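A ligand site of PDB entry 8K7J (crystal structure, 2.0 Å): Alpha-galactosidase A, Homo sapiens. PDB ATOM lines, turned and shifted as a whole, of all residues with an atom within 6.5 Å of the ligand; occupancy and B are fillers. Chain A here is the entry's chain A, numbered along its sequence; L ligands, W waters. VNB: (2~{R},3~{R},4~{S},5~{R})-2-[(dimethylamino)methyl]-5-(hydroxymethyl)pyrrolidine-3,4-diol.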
ATOM      1  N   LEU A  14      -5.242  -6.063  -4.963  1.00  0.00           N
ATOM      2  CA  LEU A  14      -5.377  -7.521  -5.008  1.00  0.00           C
ATOM      3  C   LEU A  14      -6.390  -7.908  -3.946  1.00  0.00           C
ATOM      4  O   LEU A  14      -6.284  -7.440  -2.811  1.00  0.00           O
ATOM      5  CB  LEU A  14      -4.024  -8.201  -4.734  1.00  0.00           C
ATOM      6  CG  LEU A  14      -3.983  -9.742  -4.693  1.00  0.00           C
ATOM      7  CD1 LEU A  14      -4.362 -10.320  -6.066  1.00  0.00           C
ATOM      8  CD2 LEU A  14      -2.569 -10.219  -4.264  1.00  0.00           C
ATOM      9  N   TRP A  16      -7.122 -10.579  -2.107  1.00  0.00           N
ATOM     10  CA  TRP A  16      -7.076 -11.754  -1.224  1.00  0.00           C
ATOM     11  C   TRP A  16      -7.226 -11.410   0.252  1.00  0.00           C
ATOM     12  O   TRP A  16      -8.083 -11.990   0.948  1.00  0.00           O
ATOM     13  CB  TRP A  16      -5.789 -12.541  -1.447  1.00  0.00           C
ATOM     14  CG  TRP A  16      -5.828 -13.749  -0.580  1.00  0.00           C
ATOM     15  CD1 TRP A  16      -5.098 -13.976   0.545  1.00  0.00           C
ATOM     16  CD2 TRP A  16      -6.698 -14.879  -0.739  1.00  0.00           C
ATOM     17  NE1 TRP A  16      -5.434 -15.201   1.077  1.00  0.00           N
ATOM     18  CE2 TRP A  16      -6.417 -15.773   0.301  1.00  0.00           C
ATOM     19  CE3 TRP A  16      -7.667 -15.228  -1.694  1.00  0.00           C
ATOM     20  CZ2 TRP A  16      -7.074 -17.005   0.446  1.00  0.00           C
ATOM     21  CZ3 TRP A  16      -8.327 -16.452  -1.554  1.00  0.00           C
ATOM     22  CH2 TRP A  16      -8.032 -17.328  -0.494  1.00  0.00           C
ATOM     23  N   ASP A  61      -7.267 -12.776  -7.182  1.00  0.00           N
ATOM     24  CA  ASP A  61      -6.522 -13.850  -6.528  1.00  0.00           C
ATOM     25  C   ASP A  61      -7.279 -15.151  -6.706  1.00  0.00           C
ATOM     26  O   ASP A  61      -8.028 -15.315  -7.679  1.00  0.00           O
ATOM     27  CB  ASP A  61      -6.258 -13.506  -5.045  1.00  0.00           C
ATOM     28  CG  ASP A  61      -4.976 -14.129  -4.512  1.00  0.00           C
ATOM     29  OD1 ASP A  61      -5.004 -15.338  -4.186  1.00  0.00           O
ATOM     30  OD2 ASP A  61      -3.938 -13.434  -4.420  1.00  0.00           O
ATOM     31  N   ASP A  62      -7.115 -16.099  -5.776  1.00  0.00           N
ATOM     32  CA  ASP A  62      -7.728 -17.414  -5.894  1.00  0.00           C
ATOM     33  C   ASP A  62      -9.254 -17.298  -5.858  1.00  0.00           C
ATOM     34  O   ASP A  62      -9.826 -16.269  -5.483  1.00  0.00           O
ATOM     35  CB  ASP A  62      -7.215 -18.311  -4.758  1.00  0.00           C
ATOM     36  CG  ASP A  62      -7.322 -19.802  -5.052  1.00  0.00           C
ATOM     37  OD1 ASP A  62      -7.967 -20.240  -6.024  1.00  0.00           O
ATOM     38  OD2 ASP A  62      -6.714 -20.564  -4.290  1.00  0.00           O
ATOM     39  N   CYS A  63      -9.921 -18.385  -6.247  1.00  0.00           N
ATOM     40  CA  CYS A  63     -11.377 -18.540  -6.155  1.00  0.00           C
ATOM     41  C   CYS A  63     -12.132 -17.735  -7.201  1.00  0.00           C
ATOM     42  O   CYS A  63     -13.259 -17.292  -6.969  1.00  0.00           O
ATOM     43  CB  CYS A  63     -11.902 -18.206  -4.751  1.00  0.00           C
ATOM     44  SG  CYS A  63     -11.001 -19.143  -3.509  1.00  0.00           S
ATOM     45  N   TYR A 103      -4.850 -15.156 -11.272  1.00  0.00           N
ATOM     46  CA  TYR A 103      -4.194 -16.085 -10.364  1.00  0.00           C
ATOM     47  C   TYR A 103      -4.244 -17.500 -10.934  1.00  0.00           C
ATOM     48  O   TYR A 103      -5.253 -17.904 -11.506  1.00  0.00           O
ATOM     49  CB  TYR A 103      -4.882 -16.050  -8.969  1.00  0.00           C
ATOM     50  CG  TYR A 103      -4.494 -17.164  -8.007  1.00  0.00           C
ATOM     51  CD1 TYR A 103      -5.097 -18.419  -8.093  1.00  0.00           C
ATOM     52  CD2 TYR A 103      -3.590 -16.935  -6.974  1.00  0.00           C
ATOM     53  CE1 TYR A 103      -4.760 -19.432  -7.216  1.00  0.00           C
ATOM     54  CE2 TYR A 103      -3.261 -17.950  -6.073  1.00  0.00           C
ATOM     55  CZ  TYR A 103      -3.840 -19.201  -6.212  1.00  0.00           C
ATOM     56  OH  TYR A 103      -3.537 -20.223  -5.347  1.00  0.00           O
ATOM     57  N   THR A 110      -5.239 -25.184  -7.005  1.00  0.00           N
ATOM     58  CA  THR A 110      -4.954 -23.951  -6.288  1.00  0.00           C
ATOM     59  C   THR A 110      -5.028 -24.204  -4.789  1.00  0.00           C
ATOM     60  O   THR A 110      -5.538 -25.231  -4.339  1.00  0.00           O
ATOM     61  CB  THR A 110      -5.927 -22.836  -6.677  1.00  0.00           C
ATOM     62  OG1 THR A 110      -7.222 -23.118  -6.116  1.00  0.00           O
ATOM     63  CG2 THR A 110      -6.040 -22.713  -8.215  1.00  0.00           C
ATOM     64  N   CYS A 111      -4.491 -23.266  -4.005  1.00  0.00           N
ATOM     65  CA  CYS A 111      -4.492 -23.468  -2.558  1.00  0.00           C
ATOM     66  C   CYS A 111      -5.910 -23.636  -2.026  1.00  0.00           C
ATOM     67  O   CYS A 111      -6.120 -24.345  -1.041  1.00  0.00           O
ATOM     68  CB  CYS A 111      -3.780 -22.313  -1.851  1.00  0.00           C
ATOM     69  SG  CYS A 111      -1.991 -22.220  -2.218  1.00  0.00           S
ATOM     70  N   ALA A 112      -6.901 -23.020  -2.686  1.00  0.00           N
ATOM     71  CA  ALA A 112      -8.290 -23.187  -2.282  1.00  0.00           C
ATOM     72  C   ALA A 112      -8.964 -24.397  -2.921  1.00  0.00           C
ATOM     73  O   ALA A 112     -10.149 -24.631  -2.681  1.00  0.00           O
ATOM     74  CB  ALA A 112      -9.085 -21.923  -2.613  1.00  0.00           C
ATOM     75  N   LYS A 137      -0.241 -13.931 -10.952  1.00  0.00           N
ATOM     76  CA  LYS A 137       0.267 -14.417  -9.679  1.00  0.00           C
ATOM     77  C   LYS A 137       0.149 -15.932  -9.685  1.00  0.00           C
ATOM     78  O   LYS A 137      -0.956 -16.478  -9.832  1.00  0.00           O
ATOM     79  CB  LYS A 137      -0.512 -13.817  -8.497  1.00  0.00           C
ATOM     80  CG  LYS A 137      -0.137 -14.444  -7.154  1.00  0.00           C
ATOM     81  CD  LYS A 137      -0.919 -13.835  -5.977  1.00  0.00           C
ATOM     82  CE  LYS A 137      -0.625 -14.586  -4.679  1.00  0.00           C
ATOM     83  NZ  LYS A 137      -1.398 -14.011  -3.524  1.00  0.00           N
ATOM     84  N   ASP A 139       0.784 -19.404  -7.793  1.00  0.00           N
ATOM     85  CA  ASP A 139       0.892 -19.946  -6.441  1.00  0.00           C
ATOM     86  C   ASP A 139       1.555 -21.323  -6.462  1.00  0.00           C
ATOM     87  O   ASP A 139       1.729 -21.949  -7.505  1.00  0.00           O
ATOM     88  CB  ASP A 139      -0.504 -20.021  -5.809  1.00  0.00           C
ATOM     89  CG  ASP A 139      -0.480 -19.818  -4.301  1.00  0.00           C
ATOM     90  OD1 ASP A 139       0.615 -19.885  -3.690  1.00  0.00           O
ATOM     91  OD2 ASP A 139      -1.571 -19.604  -3.722  1.00  0.00           O
ATOM     92  N   GLY A 140       1.892 -21.820  -5.269  1.00  0.00           N
ATOM     93  CA  GLY A 140       2.715 -23.017  -5.186  1.00  0.00           C
ATOM     94  C   GLY A 140       2.123 -24.229  -4.480  1.00  0.00           C
ATOM     95  O   GLY A 140       2.858 -25.192  -4.225  1.00  0.00           O
ATOM     96  N   CYS A 141       0.815 -24.224  -4.183  1.00  0.00           N
ATOM     97  CA  CYS A 141       0.218 -25.345  -3.464  1.00  0.00           C
ATOM     98  C   CYS A 141       0.104 -26.592  -4.337  1.00  0.00           C
ATOM     99  O   CYS A 141       0.055 -26.523  -5.568  1.00  0.00           O
ATOM    100  CB  CYS A 141      -1.184 -24.996  -2.949  1.00  0.00           C
ATOM    101  SG  CYS A 141      -1.199 -23.951  -1.496  1.00  0.00           S
ATOM    102  N   GLU A 172       5.479 -17.349  -6.359  1.00  0.00           N
ATOM    103  CA  GLU A 172       5.596 -17.734  -4.956  1.00  0.00           C
ATOM    104  C   GLU A 172       6.717 -18.745  -4.736  1.00  0.00           C
ATOM    105  O   GLU A 172       6.864 -19.278  -3.633  1.00  0.00           O
ATOM    106  CB  GLU A 172       4.268 -18.307  -4.445  1.00  0.00           C
ATOM    107  CG  GLU A 172       3.030 -17.468  -4.746  1.00  0.00           C
ATOM    108  CD  GLU A 172       3.086 -16.111  -4.067  1.00  0.00           C
ATOM    109  OE1 GLU A 172       3.368 -16.076  -2.854  1.00  0.00           O
ATOM    110  OE2 GLU A 172       2.838 -15.078  -4.722  1.00  0.00           O
ATOM    111  N   LEU A 175       9.327 -18.984  -1.558  1.00  0.00           N
ATOM    112  CA  LEU A 175       8.603 -19.338  -0.337  1.00  0.00           C
ATOM    113  C   LEU A 175       8.357 -20.840  -0.247  1.00  0.00           C
ATOM    114  O   LEU A 175       8.587 -21.458   0.797  1.00  0.00           O
ATOM    115  CB  LEU A 175       7.286 -18.568  -0.291  1.00  0.00           C
ATOM    116  CG  LEU A 175       6.307 -18.950   0.818  1.00  0.00           C
ATOM    117  CD1 LEU A 175       6.929 -18.758   2.194  1.00  0.00           C
ATOM    118  CD2 LEU A 175       4.991 -18.167   0.715  1.00  0.00           C
ATOM    119  N   TYR A 176       7.945 -21.460  -1.345  1.00  0.00           N
ATOM    120  CA  TYR A 176       7.680 -22.883  -1.296  1.00  0.00           C
ATOM    121  C   TYR A 176       8.947 -23.711  -1.361  1.00  0.00           C
ATOM    122  O   TYR A 176       8.918 -24.890  -0.985  1.00  0.00           O
ATOM    123  CB  TYR A 176       6.723 -23.274  -2.420  1.00  0.00           C
ATOM    124  CG  TYR A 176       5.308 -22.821  -2.141  1.00  0.00           C
ATOM    125  CD1 TYR A 176       4.884 -21.531  -2.473  1.00  0.00           C
ATOM    126  CD2 TYR A 176       4.396 -23.660  -1.509  1.00  0.00           C
ATOM    127  CE1 TYR A 176       3.585 -21.107  -2.206  1.00  0.00           C
ATOM    128  CE2 TYR A 176       3.087 -23.250  -1.237  1.00  0.00           C
ATOM    129  CZ  TYR A 176       2.691 -21.968  -1.582  1.00  0.00           C
ATOM    130  OH  TYR A 176       1.398 -21.574  -1.308  1.00  0.00           O
ATOM    131  N   ARG A 196       7.820 -14.032  -3.948  1.00  0.00           N
ATOM    132  CA  ARG A 196       7.524 -14.020  -2.526  1.00  0.00           C
ATOM    133  C   ARG A 196       8.520 -14.860  -1.744  1.00  0.00           C
ATOM    134  O   ARG A 196       8.770 -16.021  -2.104  1.00  0.00           O
ATOM    135  CB  ARG A 196       6.110 -14.516  -2.266  1.00  0.00           C
ATOM    136  CG  ARG A 196       5.858 -14.673  -0.786  1.00  0.00           C
ATOM    137  CD  ARG A 196       5.222 -13.423  -0.258  1.00  0.00           C
ATOM    138  NE  ARG A 196       3.821 -13.464  -0.629  1.00  0.00           N
ATOM    139  CZ  ARG A 196       2.911 -14.172  -0.008  1.00  0.00           C
ATOM    140  NH1 ARG A 196       3.199 -14.887   1.079  1.00  0.00           N
ATOM    141  NH2 ARG A 196       1.683 -14.252  -0.516  1.00  0.00           N
ATOM    142  N   PHE A 198       8.366 -14.950   1.998  1.00  0.00           N
ATOM    143  CA  PHE A 198       7.966 -15.195   3.374  1.00  0.00           C
ATOM    144  C   PHE A 198       6.455 -15.414   3.441  1.00  0.00           C
ATOM    145  O   PHE A 198       5.739 -15.202   2.471  1.00  0.00           O
ATOM    146  CB  PHE A 198       8.378 -14.017   4.263  1.00  0.00           C
ATOM    147  CG  PHE A 198       9.854 -13.673   4.185  1.00  0.00           C
ATOM    148  CD1 PHE A 198      10.847 -14.652   4.301  1.00  0.00           C
ATOM    149  CD2 PHE A 198      10.254 -12.356   3.997  1.00  0.00           C
ATOM    150  CE1 PHE A 198      12.221 -14.308   4.236  1.00  0.00           C
ATOM    151  CE2 PHE A 198      11.609 -12.002   3.922  1.00  0.00           C
ATOM    152  CZ  PHE A 198      12.590 -12.973   4.039  1.00  0.00           C
ATOM    153  N   ALA A 199       5.971 -15.825   4.615  1.00  0.00           N
ATOM    154  CA  ALA A 199       4.591 -16.265   4.754  1.00  0.00           C
ATOM    155  C   ALA A 199       3.618 -15.099   4.518  1.00  0.00           C
ATOM    156  O   ALA A 199       3.996 -13.920   4.515  1.00  0.00           O
ATOM    157  CB  ALA A 199       4.367 -16.870   6.144  1.00  0.00           C
ATOM    158  N   ASP A 200       2.343 -15.463   4.346  1.00  0.00           N
ATOM    159  CA  ASP A 200       1.298 -14.499   4.007  1.00  0.00           C
ATOM    160  C   ASP A 200       1.152 -13.436   5.080  1.00  0.00           C
ATOM    161  O   ASP A 200       1.203 -13.723   6.275  1.00  0.00           O
ATOM    162  CB  ASP A 200      -0.071 -15.180   3.851  1.00  0.00           C
ATOM    163  CG  ASP A 200      -0.150 -16.101   2.661  1.00  0.00           C
ATOM    164  OD1 ASP A 200       0.807 -16.136   1.851  1.00  0.00           O
ATOM    165  OD2 ASP A 200      -1.206 -16.753   2.528  1.00  0.00           O
ATOM    166  N   ASP A 235       4.594  -9.175   0.274  1.00  0.00           N
ATOM    167  CA  ASP A 235       3.141  -9.361   0.269  1.00  0.00           C
ATOM    168  C   ASP A 235       2.391  -8.023   0.373  1.00  0.00           C
ATOM    169  O   ASP A 235       2.998  -6.948   0.359  1.00  0.00           O
ATOM    170  CB  ASP A 235       2.697 -10.333   1.384  1.00  0.00           C
ATOM    171  CG  ASP A 235       1.443 -11.137   1.012  1.00  0.00           C
ATOM    172  OD1 ASP A 235       0.888 -10.886  -0.077  1.00  0.00           O
ATOM    173  OD2 ASP A 235       0.994 -12.015   1.802  1.00  0.00           O
ATOM    174  N   MET A 236       1.064  -8.104   0.473  1.00  0.00           N
ATOM    175  CA  MET A 236       0.165  -6.978   0.218  1.00  0.00           C
ATOM    176  C   MET A 236       0.287  -5.886   1.286  1.00  0.00           C
ATOM    177  O   MET A 236       0.647  -6.142   2.429  1.00  0.00           O
ATOM    178  CB  MET A 236      -1.277  -7.467   0.171  1.00  0.00           C
ATOM    179  CG  MET A 236      -1.626  -8.394  -1.016  1.00  0.00           C
ATOM    180  SD  MET A 236      -3.128  -9.344  -0.682  1.00  0.00           S
ATOM    181  CE  MET A 236      -2.431 -10.657   0.342  1.00  0.00           C
HETATM  182  CAA VNB L   1       1.457 -17.906  -1.102  1.00  0.00           C
HETATM  183  CAB VNB L   1      -3.847 -17.831  -1.277  1.00  0.00           C
HETATM  184  CAC VNB L   1      -3.266 -16.442  -1.370  1.00  0.00           C
HETATM  185  CAD VNB L   1      -1.995 -16.621  -0.572  1.00  0.00           C
HETATM  186  CAE VNB L   1      -1.477 -17.952  -1.109  1.00  0.00           C
HETATM  187  CAG VNB L   1      -4.854 -18.032  -2.398  1.00  0.00           C
HETATM  188  CAK VNB L   1      -0.635 -18.739  -0.097  1.00  0.00           C
HETATM  189  CAM VNB L   1       1.471 -19.110   0.972  1.00  0.00           C
HETATM  190  NAF VNB L   1      -2.690 -18.731  -1.426  1.00  0.00           N
HETATM  191  NAL VNB L   1       0.697 -18.152   0.139  1.00  0.00           N
HETATM  192  OAH VNB L   1      -2.941 -16.203  -2.764  1.00  0.00           O
HETATM  193  OAI VNB L   1      -1.084 -15.553  -0.830  1.00  0.00           O
HETATM  194  OAJ VNB L   1      -5.484 -19.307  -2.219  1.00  0.00           O
HETATM  195  O   HOH W   1      -6.596 -20.584   0.094  1.00  0.00           O
HETATM  196  O   HOH W   2      -1.091 -13.502   1.010  1.00  0.00           O
HETATM  197  O   HOH W   3      -3.406 -20.363   0.827  1.00  0.00           O
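OD1 of Asp 200 is in salt-bridge range of NAL of the ligand (2.6 Å).
OD1 of Asp 61 sits at hydrogen-bond distance from OAH of the ligand (2.7 Å).
The side-chain carboxylate (OD2) of Asp 139 lies within salt-bridge range of a nitrogen (NAF) of the ligand (2.7 Å).
OD2 of Asp 62 sits at hydrogen-bond distance from OAJ of the ligand (2.7 Å).
NZ of Lys 137 sits at hydrogen-bond distance from OAH of the ligand (2.8 Å).
The guanidinium group (NH2) of Arg 196 lies within hydrogen-bond range of an oxygen (OAI) of the ligand.
SG of Cys 111 sits at hydrogen-bond distance from NAF of the ligand, 3.6 Å away.
OD1 of Asp 200 lies within salt-bridge range of NH1 of Arg 196 (2.8 Å).
OD2 of Asp 61 lies within salt-bridge range of NZ of Lys 137.
The side-chain hydroxyl (OG1) of Thr 110 is in hydrogen-bond range of the side-chain carboxylate (OD1) of Asp 62 (3.0 Å).
The guanidinium group (NH2) of Arg 196 lies within salt-bridge range of the side-chain carboxylate (OD2) of Asp 235 (3.3 Å).
O of Phe 198 sits at hydrogen-bond distance from NH1 of Arg 196.
The side-chain hydroxyl (OH) of Tyr 176 sits at hydrogen-bond distance from the side-chain sulfur (SG) of Cys 111 (3.6 Å).
The side-chain hydroxyl (OH) of Tyr 176 lies within hydrogen-bond range of the side-chain sulfur (SG) of Cys 141, 3.5 Å away.
The backbone NH of Cys 111 sits at hydrogen-bond distance from the side-chain hydroxyl of Tyr 103 (3.5 Å).
Residues that only touch the ligand: Glu 172, Tyr 176, Trp 16, Leu 175 and Tyr 103.
Hydrophobic or aromatic side chains that line the ligand: Trp 16, Tyr 103, Leu 175 and Tyr 176.
Within 4 Å of the ligand: Trp 16, Asp 61, Asp 62, Tyr 103, Cys 111, Lys 137, Asp 139, Glu 172, Leu 175, Tyr 176, Arg 196 and Asp 200.
The nearest printed residue that does not touch the ligand is Ala 112 (4.002 Å).
Water W2 lies within hydrogen-bond range of the side-chain carboxylate (OD2) of Asp 235 (2.7 Å), an oxygen (OAI) of the ligand (2.8 Å), the guanidinium group (NH2) of Arg 196 (3.3 Å) and the side-chain carboxylate (OD1) of Asp 200 (3.4 Å).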
